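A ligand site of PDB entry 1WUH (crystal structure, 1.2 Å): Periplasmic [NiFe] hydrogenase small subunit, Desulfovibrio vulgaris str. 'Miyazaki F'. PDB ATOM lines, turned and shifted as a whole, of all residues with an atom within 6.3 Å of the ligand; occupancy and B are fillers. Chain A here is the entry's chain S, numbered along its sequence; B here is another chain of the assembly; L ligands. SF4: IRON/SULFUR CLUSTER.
An iron atom (FE4) of the ligand is bound by the side-chain sulfur (SG) of Cys 20 (2.2 Å).
A sulfur (S1) of the ligand sits close to the backbone NH of Cys 114, at 3.5 Å.
The side-chain sulfur of Cys 114 is bound to an iron atom (FE2) of the ligand, 2.3 Å away.
A sulfur (S3) of the ligand sits close to the backbone NH (N) of Cys 17.
SG of Cys 17 binds FE1 of the ligand, at 2.3 Å.
The side-chain sulfur (SG) of Cys 150 binds an iron atom (FE3) of the ligand (2.3 Å).
The backbone NH (N) of Thr 113 lies close to a sulfur (S1) of the ligand (3.4 Å).
A ring nitrogen (ND1) of His 217 of chain B sits close to a sulfur (S2) of the ligand (3.7 Å).
SG of Cys 20 lies close to O of Tyr 111 (3.7 Å).
N of Val 120 sits close to SG of Cys 114, 3.8 Å away.
The side-chain amide nitrogen of Gln 121 lies close to the side-chain sulfur of Cys 114 (3.3 Å).
The backbone carbonyl oxygen of Cys 17 lies within hydrogen-bond range of the backbone NH of Gly 64 of chain B (2.8 Å).
The backbone NH (N) of Thr 113 is in hydrogen-bond range of the backbone carbonyl oxygen (O) of Gly 149 (2.9 Å).
The side-chain hydroxyl (OG1) of Thr 18 is in hydrogen-bond range of the side-chain carboxylate (OE1) of Glu 16.
The backbone NH (N) of Thr 18 sits close to the side-chain carboxylate (OE1) of Glu 75, 3.4 Å away.
The side-chain carboxylate (OE2) of Glu 75 is in hydrogen-bond range of the side-chain hydroxyl (OG) of Ser 21 (2.6 Å).
A sulfur (S1) of the ligand lies close to the backbone carbonyl oxygen of Gly 149 (3.6 Å).
The backbone nitrogen of Pro 151 lies close to a sulfur (S2) of the ligand (3.6 Å).
Glu 16 touches the ligand.
CA of Gly 19 touches S2 of the ligand, at 3.9 Å.
OE1 of Glu 75 touches S3 of the ligand, 3.9 Å away.
Gly 112 touches the ligand.
Arg 61 of chain B touches the ligand (CG to S4, 3.4 Å).
Hydrophobic or aromatic side chains that line the ligand: Pro 151 and His 217 of chain B.
13 residues have an atom within 4 Å of the ligand: Glu 16, Cys 17, Gly 19, Cys 20, Glu 75, Gly 112, Thr 113, Cys 114, Gly 149, Cys 150, Pro 151, Arg 61 of chain B and His 217 of chain B.
The nearest printed residue that does not touch the ligand is Val 120 (4.04 Å).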
ATOM      1  N   ALA A  15     -18.909 -26.114  -9.949  1.00  0.00           N
ATOM      2  CA  ALA A  15     -18.882 -26.883 -11.177  1.00  0.00           C
ATOM      3  C   ALA A  15     -18.414 -25.926 -12.254  1.00  0.00           C
ATOM      4  O   ALA A  15     -19.219 -25.148 -12.764  1.00  0.00           O
ATOM      5  CB  ALA A  15     -20.230 -27.497 -11.460  1.00  0.00           C
ATOM      6  N   GLU A  16     -17.129 -26.020 -12.546  1.00  0.00           N
ATOM      7  CA  GLU A  16     -16.469 -25.034 -13.390  1.00  0.00           C
ATOM      8  C   GLU A  16     -15.351 -25.693 -14.168  1.00  0.00           C
ATOM      9  O   GLU A  16     -14.947 -26.784 -13.894  1.00  0.00           O
ATOM     10  CB  GLU A  16     -15.975 -23.859 -12.532  1.00  0.00           C
ATOM     11  CG  GLU A  16     -15.276 -24.220 -11.252  1.00  0.00           C
ATOM     12  CD  GLU A  16     -13.838 -24.675 -11.374  1.00  0.00           C
ATOM     13  OE1 GLU A  16     -13.109 -24.059 -12.188  1.00  0.00           O
ATOM     14  OE2 GLU A  16     -13.440 -25.577 -10.591  1.00  0.00           O
ATOM     15  N   CYS A  17     -14.871 -24.940 -15.177  1.00  0.00           N
ATOM     16  CA  CYS A  17     -13.793 -25.385 -16.025  1.00  0.00           C
ATOM     17  C   CYS A  17     -12.486 -24.662 -15.771  1.00  0.00           C
ATOM     18  O   CYS A  17     -11.475 -24.943 -16.393  1.00  0.00           O
ATOM     19  CB  CYS A  17     -14.180 -25.235 -17.509  1.00  0.00           C
ATOM     20  SG  CYS A  17     -13.960 -23.568 -18.216  1.00  0.00           S
ATOM     21  N   THR A  18     -12.535 -23.672 -14.877  1.00  0.00           N
ATOM     22  CA  THR A  18     -11.380 -22.860 -14.444  1.00  0.00           C
ATOM     23  C   THR A  18     -11.051 -21.802 -15.492  1.00  0.00           C
ATOM     24  O   THR A  18     -10.135 -21.011 -15.344  1.00  0.00           O
ATOM     25  CB  THR A  18     -10.182 -23.722 -13.980  1.00  0.00           C
ATOM     26  OG1 THR A  18     -10.752 -24.744 -13.087  1.00  0.00           O
ATOM     27  CG2 THR A  18      -9.129 -22.995 -13.205  1.00  0.00           C
ATOM     28  N   GLY A  19     -11.857 -21.749 -16.574  1.00  0.00           N
ATOM     29  CA  GLY A  19     -11.682 -20.687 -17.543  1.00  0.00           C
ATOM     30  C   GLY A  19     -11.948 -19.294 -17.015  1.00  0.00           C
ATOM     31  O   GLY A  19     -11.350 -18.309 -17.450  1.00  0.00           O
ATOM     32  N   CYS A  20     -12.883 -19.189 -16.076  1.00  0.00           N
ATOM     33  CA  CYS A  20     -13.110 -17.880 -15.463  1.00  0.00           C
ATOM     34  C   CYS A  20     -11.928 -17.489 -14.598  1.00  0.00           C
ATOM     35  O   CYS A  20     -11.463 -16.338 -14.679  1.00  0.00           O
ATOM     36  CB  CYS A  20     -14.439 -17.891 -14.670  1.00  0.00           C
ATOM     37  SG  CYS A  20     -15.898 -17.937 -15.757  1.00  0.00           S
ATOM     38  N   SER A  21     -11.355 -18.381 -13.795  1.00  0.00           N
ATOM     39  CA  SER A  21     -10.148 -18.028 -13.076  1.00  0.00           C
ATOM     40  C   SER A  21      -9.038 -17.628 -14.022  1.00  0.00           C
ATOM     41  O   SER A  21      -8.336 -16.664 -13.779  1.00  0.00           O
ATOM     42  CB  SER A  21      -9.607 -19.215 -12.249  1.00  0.00           C
ATOM     43  OG  SER A  21     -10.351 -19.484 -11.086  1.00  0.00           O
ATOM     44  N   GLU A  75     -17.090 -18.938  -8.958  1.00  0.00           N
ATOM     45  CA  GLU A  75     -16.956 -19.509 -10.279  1.00  0.00           C
ATOM     46  C   GLU A  75     -17.621 -20.883 -10.323  1.00  0.00           C
ATOM     47  O   GLU A  75     -17.385 -21.668  -9.410  1.00  0.00           O
ATOM     48  CB  GLU A  75     -15.459 -19.649 -10.609  1.00  0.00           C
ATOM     49  CG  GLU A  75     -15.153 -20.290 -11.949  1.00  0.00           C
ATOM     50  CD  GLU A  75     -13.688 -20.189 -12.305  1.00  0.00           C
ATOM     51  OE1 GLU A  75     -13.278 -20.649 -13.410  1.00  0.00           O
ATOM     52  OE2 GLU A  75     -12.910 -19.689 -11.453  1.00  0.00           O
ATOM     53  N   GLY A  76     -18.484 -21.138 -11.304  1.00  0.00           N
ATOM     54  CA  GLY A  76     -19.118 -22.404 -11.474  1.00  0.00           C
ATOM     55  C   GLY A  76     -20.550 -22.479 -10.992  1.00  0.00           C
ATOM     56  O   GLY A  76     -20.968 -21.776 -10.081  1.00  0.00           O
ATOM     57  N   GLY A  77     -21.321 -23.380 -11.604  1.00  0.00           N
ATOM     58  CA  GLY A  77     -22.651 -23.676 -11.156  1.00  0.00           C
ATOM     59  C   GLY A  77     -22.642 -24.585  -9.948  1.00  0.00           C
ATOM     60  O   GLY A  77     -21.672 -25.275  -9.669  1.00  0.00           O
ATOM     61  N   TYR A 111     -19.243 -14.984 -11.007  1.00  0.00           N
ATOM     62  CA  TYR A 111     -18.370 -14.662 -12.118  1.00  0.00           C
ATOM     63  C   TYR A 111     -18.389 -15.816 -13.119  1.00  0.00           C
ATOM     64  O   TYR A 111     -17.957 -16.927 -12.798  1.00  0.00           O
ATOM     65  CB  TYR A 111     -16.939 -14.366 -11.591  1.00  0.00           C
ATOM     66  CG  TYR A 111     -15.998 -13.895 -12.696  1.00  0.00           C
ATOM     67  CD1 TYR A 111     -16.294 -12.743 -13.409  1.00  0.00           C
ATOM     68  CD2 TYR A 111     -14.862 -14.619 -13.019  1.00  0.00           C
ATOM     69  CE1 TYR A 111     -15.470 -12.268 -14.416  1.00  0.00           C
ATOM     70  CE2 TYR A 111     -14.053 -14.166 -14.039  1.00  0.00           C
ATOM     71  CZ  TYR A 111     -14.345 -13.023 -14.750  1.00  0.00           C
ATOM     72  OH  TYR A 111     -13.557 -12.527 -15.783  1.00  0.00           O
ATOM     73  N   GLY A 112     -18.916 -15.507 -14.308  1.00  0.00           N
ATOM     74  CA  GLY A 112     -19.090 -16.398 -15.409  1.00  0.00           C
ATOM     75  C   GLY A 112     -20.492 -16.944 -15.511  1.00  0.00           C
ATOM     76  O   GLY A 112     -21.208 -17.101 -14.538  1.00  0.00           O
ATOM     77  N   THR A 113     -20.869 -17.266 -16.724  1.00  0.00           N
ATOM     78  CA  THR A 113     -22.211 -17.816 -16.995  1.00  0.00           C
ATOM     79  C   THR A 113     -22.589 -19.007 -16.187  1.00  0.00           C
ATOM     80  O   THR A 113     -23.760 -19.157 -15.862  1.00  0.00           O
ATOM     81  CB  THR A 113     -22.310 -18.106 -18.511  1.00  0.00           C
ATOM     82  OG1 THR A 113     -22.261 -16.833 -19.097  1.00  0.00           O
ATOM     83  CG2 THR A 113     -23.653 -18.682 -18.919  1.00  0.00           C
ATOM     84  N   CYS A 114     -21.628 -19.860 -15.861  1.00  0.00           N
ATOM     85  CA  CYS A 114     -21.960 -20.976 -14.984  1.00  0.00           C
ATOM     86  C   CYS A 114     -22.464 -20.504 -13.618  1.00  0.00           C
ATOM     87  O   CYS A 114     -23.520 -20.938 -13.153  1.00  0.00           O
ATOM     88  CB  CYS A 114     -20.787 -21.926 -14.764  1.00  0.00           C
ATOM     89  SG  CYS A 114     -20.249 -22.772 -16.306  1.00  0.00           S
ATOM     90  N   ALA A 115     -21.680 -19.642 -12.964  1.00  0.00           N
ATOM     91  CA  ALA A 115     -22.109 -19.123 -11.687  1.00  0.00           C
ATOM     92  C   ALA A 115     -23.340 -18.254 -11.808  1.00  0.00           C
ATOM     93  O   ALA A 115     -24.183 -18.210 -10.876  1.00  0.00           O
ATOM     94  CB  ALA A 115     -20.999 -18.317 -11.021  1.00  0.00           C
ATOM     95  N   GLY A 119     -24.906 -22.404 -16.668  1.00  0.00           N
ATOM     96  CA  GLY A 119     -23.871 -22.695 -17.632  1.00  0.00           C
ATOM     97  C   GLY A 119     -23.861 -24.063 -18.239  1.00  0.00           C
ATOM     98  O   GLY A 119     -24.892 -24.708 -18.361  1.00  0.00           O
ATOM     99  N   VAL A 120     -22.669 -24.496 -18.648  1.00  0.00           N
ATOM    100  CA  VAL A 120     -22.594 -25.607 -19.571  1.00  0.00           C
ATOM    101  C   VAL A 120     -23.134 -26.900 -18.936  1.00  0.00           C
ATOM    102  O   VAL A 120     -23.821 -27.660 -19.602  1.00  0.00           O
ATOM    103  CB  VAL A 120     -21.168 -25.784 -20.085  1.00  0.00           C
ATOM    104  CG1 VAL A 120     -20.148 -26.231 -19.024  1.00  0.00           C
ATOM    105  CG2 VAL A 120     -21.109 -26.715 -21.289  1.00  0.00           C
ATOM    106  N   GLN A 121     -22.861 -27.148 -17.658  1.00  0.00           N
ATOM    107  CA  GLN A 121     -23.358 -28.366 -17.036  1.00  0.00           C
ATOM    108  C   GLN A 121     -24.865 -28.289 -16.792  1.00  0.00           C
ATOM    109  O   GLN A 121     -25.498 -29.317 -16.540  1.00  0.00           O
ATOM    110  CB  GLN A 121     -22.601 -28.710 -15.753  1.00  0.00           C
ATOM    111  CG  GLN A 121     -22.579 -27.623 -14.712  1.00  0.00           C
ATOM    112  CD  GLN A 121     -21.467 -26.640 -14.931  1.00  0.00           C
ATOM    113  OE1 GLN A 121     -20.336 -27.017 -15.228  1.00  0.00           O
ATOM    114  NE2 GLN A 121     -21.729 -25.348 -14.832  1.00  0.00           N
ATOM    115  N   GLY A 149     -20.671 -14.143 -19.182  1.00  0.00           N
ATOM    116  CA  GLY A 149     -19.759 -14.578 -20.202  1.00  0.00           C
ATOM    117  C   GLY A 149     -19.081 -15.907 -19.903  1.00  0.00           C
ATOM    118  O   GLY A 149     -19.013 -16.371 -18.763  1.00  0.00           O
ATOM    119  N   CYS A 150     -18.508 -16.492 -20.959  1.00  0.00           N
ATOM    120  CA  CYS A 150     -17.958 -17.851 -20.843  1.00  0.00           C
ATOM    121  C   CYS A 150     -16.561 -17.981 -21.473  1.00  0.00           C
ATOM    122  O   CYS A 150     -16.347 -18.618 -22.498  1.00  0.00           O
ATOM    123  CB  CYS A 150     -18.938 -18.852 -21.449  1.00  0.00           C
ATOM    124  SG  CYS A 150     -18.666 -20.586 -21.077  1.00  0.00           S
ATOM    125  N   PRO A 151     -15.554 -17.363 -20.853  1.00  0.00           N
ATOM    126  CA  PRO A 151     -15.652 -16.559 -19.622  1.00  0.00           C
ATOM    127  C   PRO A 151     -15.921 -15.097 -19.905  1.00  0.00           C
ATOM    128  O   PRO A 151     -15.859 -14.629 -21.052  1.00  0.00           O
ATOM    129  CB  PRO A 151     -14.271 -16.744 -19.007  1.00  0.00           C
ATOM    130  CG  PRO A 151     -13.379 -16.764 -20.239  1.00  0.00           C
ATOM    131  CD  PRO A 151     -14.164 -17.525 -21.286  1.00  0.00           C
ATOM    132  N   PRO A 152     -16.270 -14.371 -18.858  1.00  0.00           N
ATOM    133  CA  PRO A 152     -16.486 -12.924 -18.993  1.00  0.00           C
ATOM    134  C   PRO A 152     -15.184 -12.245 -19.331  1.00  0.00           C
ATOM    135  O   PRO A 152     -14.087 -12.752 -19.193  1.00  0.00           O
ATOM    136  CB  PRO A 152     -16.927 -12.480 -17.591  1.00  0.00           C
ATOM    137  CG  PRO A 152     -17.367 -13.739 -16.928  1.00  0.00           C
ATOM    138  CD  PRO A 152     -16.411 -14.783 -17.442  1.00  0.00           C
ATOM    139  N   TRP A 258     -26.633 -22.326 -24.028  1.00  0.00           N
ATOM    140  CA  TRP A 258     -26.302 -23.614 -24.620  1.00  0.00           C
ATOM    141  C   TRP A 258     -27.500 -24.232 -25.325  1.00  0.00           C
ATOM    142  O   TRP A 258     -27.386 -24.931 -26.317  1.00  0.00           O
ATOM    143  CB  TRP A 258     -25.771 -24.573 -23.525  1.00  0.00           C
ATOM    144  CG  TRP A 258     -24.490 -24.040 -22.945  1.00  0.00           C
ATOM    145  CD1 TRP A 258     -24.355 -23.448 -21.736  1.00  0.00           C
ATOM    146  CD2 TRP A 258     -23.203 -24.030 -23.537  1.00  0.00           C
ATOM    147  NE1 TRP A 258     -23.031 -23.063 -21.542  1.00  0.00           N
ATOM    148  CE2 TRP A 258     -22.334 -23.417 -22.639  1.00  0.00           C
ATOM    149  CE3 TRP A 258     -22.721 -24.476 -24.764  1.00  0.00           C
ATOM    150  CZ2 TRP A 258     -20.968 -23.240 -22.918  1.00  0.00           C
ATOM    151  CZ3 TRP A 258     -21.385 -24.303 -25.041  1.00  0.00           C
ATOM    152  CH2 TRP A 258     -20.525 -23.691 -24.131  1.00  0.00           C
ATOM    153  N   ARG B  41     -19.636 -33.302 -14.276  1.00  0.00           N
ATOM    154  CA  ARG B  41     -20.502 -32.380 -15.033  1.00  0.00           C
ATOM    155  C   ARG B  41     -21.332 -33.140 -16.079  1.00  0.00           C
ATOM    156  O   ARG B  41     -22.473 -32.790 -16.294  1.00  0.00           O
ATOM    157  CB  ARG B  41     -19.704 -31.250 -15.675  1.00  0.00           C
ATOM    158  CG  ARG B  41     -19.199 -30.286 -14.642  1.00  0.00           C
ATOM    159  CD  ARG B  41     -18.245 -29.200 -15.133  1.00  0.00           C
ATOM    160  NE  ARG B  41     -17.088 -29.863 -15.693  1.00  0.00           N
ATOM    161  CZ  ARG B  41     -16.343 -29.373 -16.669  1.00  0.00           C
ATOM    162  NH1 ARG B  41     -16.507 -28.182 -17.223  1.00  0.00           N
ATOM    163  NH2 ARG B  41     -15.357 -30.118 -17.146  1.00  0.00           N
ATOM    164  N   ARG B  61     -15.439 -26.109 -23.157  1.00  0.00           N
ATOM    165  CA  ARG B  61     -15.717 -25.861 -21.758  1.00  0.00           C
ATOM    166  C   ARG B  61     -15.503 -27.041 -20.824  1.00  0.00           C
ATOM    167  O   ARG B  61     -15.758 -26.951 -19.631  1.00  0.00           O
ATOM    168  CB  ARG B  61     -17.151 -25.304 -21.603  1.00  0.00           C
ATOM    169  CG  ARG B  61     -17.269 -23.823 -21.919  1.00  0.00           C
ATOM    170  CD  ARG B  61     -16.981 -23.508 -23.366  1.00  0.00           C
ATOM    171  NE  ARG B  61     -17.160 -22.078 -23.592  1.00  0.00           N
ATOM    172  CZ  ARG B  61     -16.988 -21.495 -24.767  1.00  0.00           C
ATOM    173  NH1 ARG B  61     -16.761 -22.231 -25.846  1.00  0.00           N
ATOM    174  NH2 ARG B  61     -17.072 -20.173 -24.841  1.00  0.00           N
ATOM    175  N   GLY B  64     -10.701 -24.752 -19.065  1.00  0.00           N
ATOM    176  CA  GLY B  64     -10.235 -23.409 -19.420  1.00  0.00           C
ATOM    177  C   GLY B  64      -8.762 -23.223 -19.124  1.00  0.00           C
ATOM    178  O   GLY B  64      -8.240 -22.189 -19.497  1.00  0.00           O
ATOM    179  N   PRO B 216      -9.313 -16.740 -22.315  1.00  0.00           N
ATOM    180  CA  PRO B 216      -9.664 -18.114 -22.592  1.00  0.00           C
ATOM    181  C   PRO B 216     -10.812 -18.219 -23.562  1.00  0.00           C
ATOM    182  O   PRO B 216     -11.673 -17.410 -23.807  1.00  0.00           O
ATOM    183  CB  PRO B 216     -10.055 -18.709 -21.237  1.00  0.00           C
ATOM    184  CG  PRO B 216      -9.470 -17.779 -20.218  1.00  0.00           C
ATOM    185  CD  PRO B 216      -9.561 -16.426 -20.895  1.00  0.00           C
ATOM    186  N   HIS B 217     -10.858 -19.330 -24.219  1.00  0.00           N
ATOM    187  CA  HIS B 217     -11.852 -20.084 -24.989  1.00  0.00           C
ATOM    188  C   HIS B 217     -11.885 -19.433 -26.351  1.00  0.00           C
ATOM    189  O   HIS B 217     -12.623 -18.520 -26.642  1.00  0.00           O
ATOM    190  CB  HIS B 217     -13.192 -20.159 -24.292  1.00  0.00           C
ATOM    191  CG  HIS B 217     -13.208 -21.174 -23.177  1.00  0.00           C
ATOM    192  ND1 HIS B 217     -14.111 -21.259 -22.153  1.00  0.00           N
ATOM    193  CD2 HIS B 217     -12.314 -22.216 -23.012  1.00  0.00           C
ATOM    194  CE1 HIS B 217     -13.775 -22.333 -21.391  1.00  0.00           C
ATOM    195  NE2 HIS B 217     -12.676 -22.900 -21.914  1.00  0.00           N
HETATM  196 FE1  SF4 L   1     -15.796 -22.321 -17.741  1.00  0.00          FE
HETATM  197 FE2  SF4 L   1     -18.257 -21.830 -16.781  1.00  0.00          FE
HETATM  198 FE3  SF4 L   1     -17.526 -20.800 -19.099  1.00  0.00          FE
HETATM  199 FE4  SF4 L   1     -16.385 -19.836 -16.814  1.00  0.00          FE
HETATM  200  S1  SF4 L   1     -18.534 -19.630 -17.411  1.00  0.00           S
HETATM  201  S2  SF4 L   1     -15.367 -20.324 -18.834  1.00  0.00           S
HETATM  202  S3  SF4 L   1     -16.358 -21.772 -15.551  1.00  0.00           S
HETATM  203  S4  SF4 L   1     -17.689 -23.057 -18.610  1.00  0.00           S
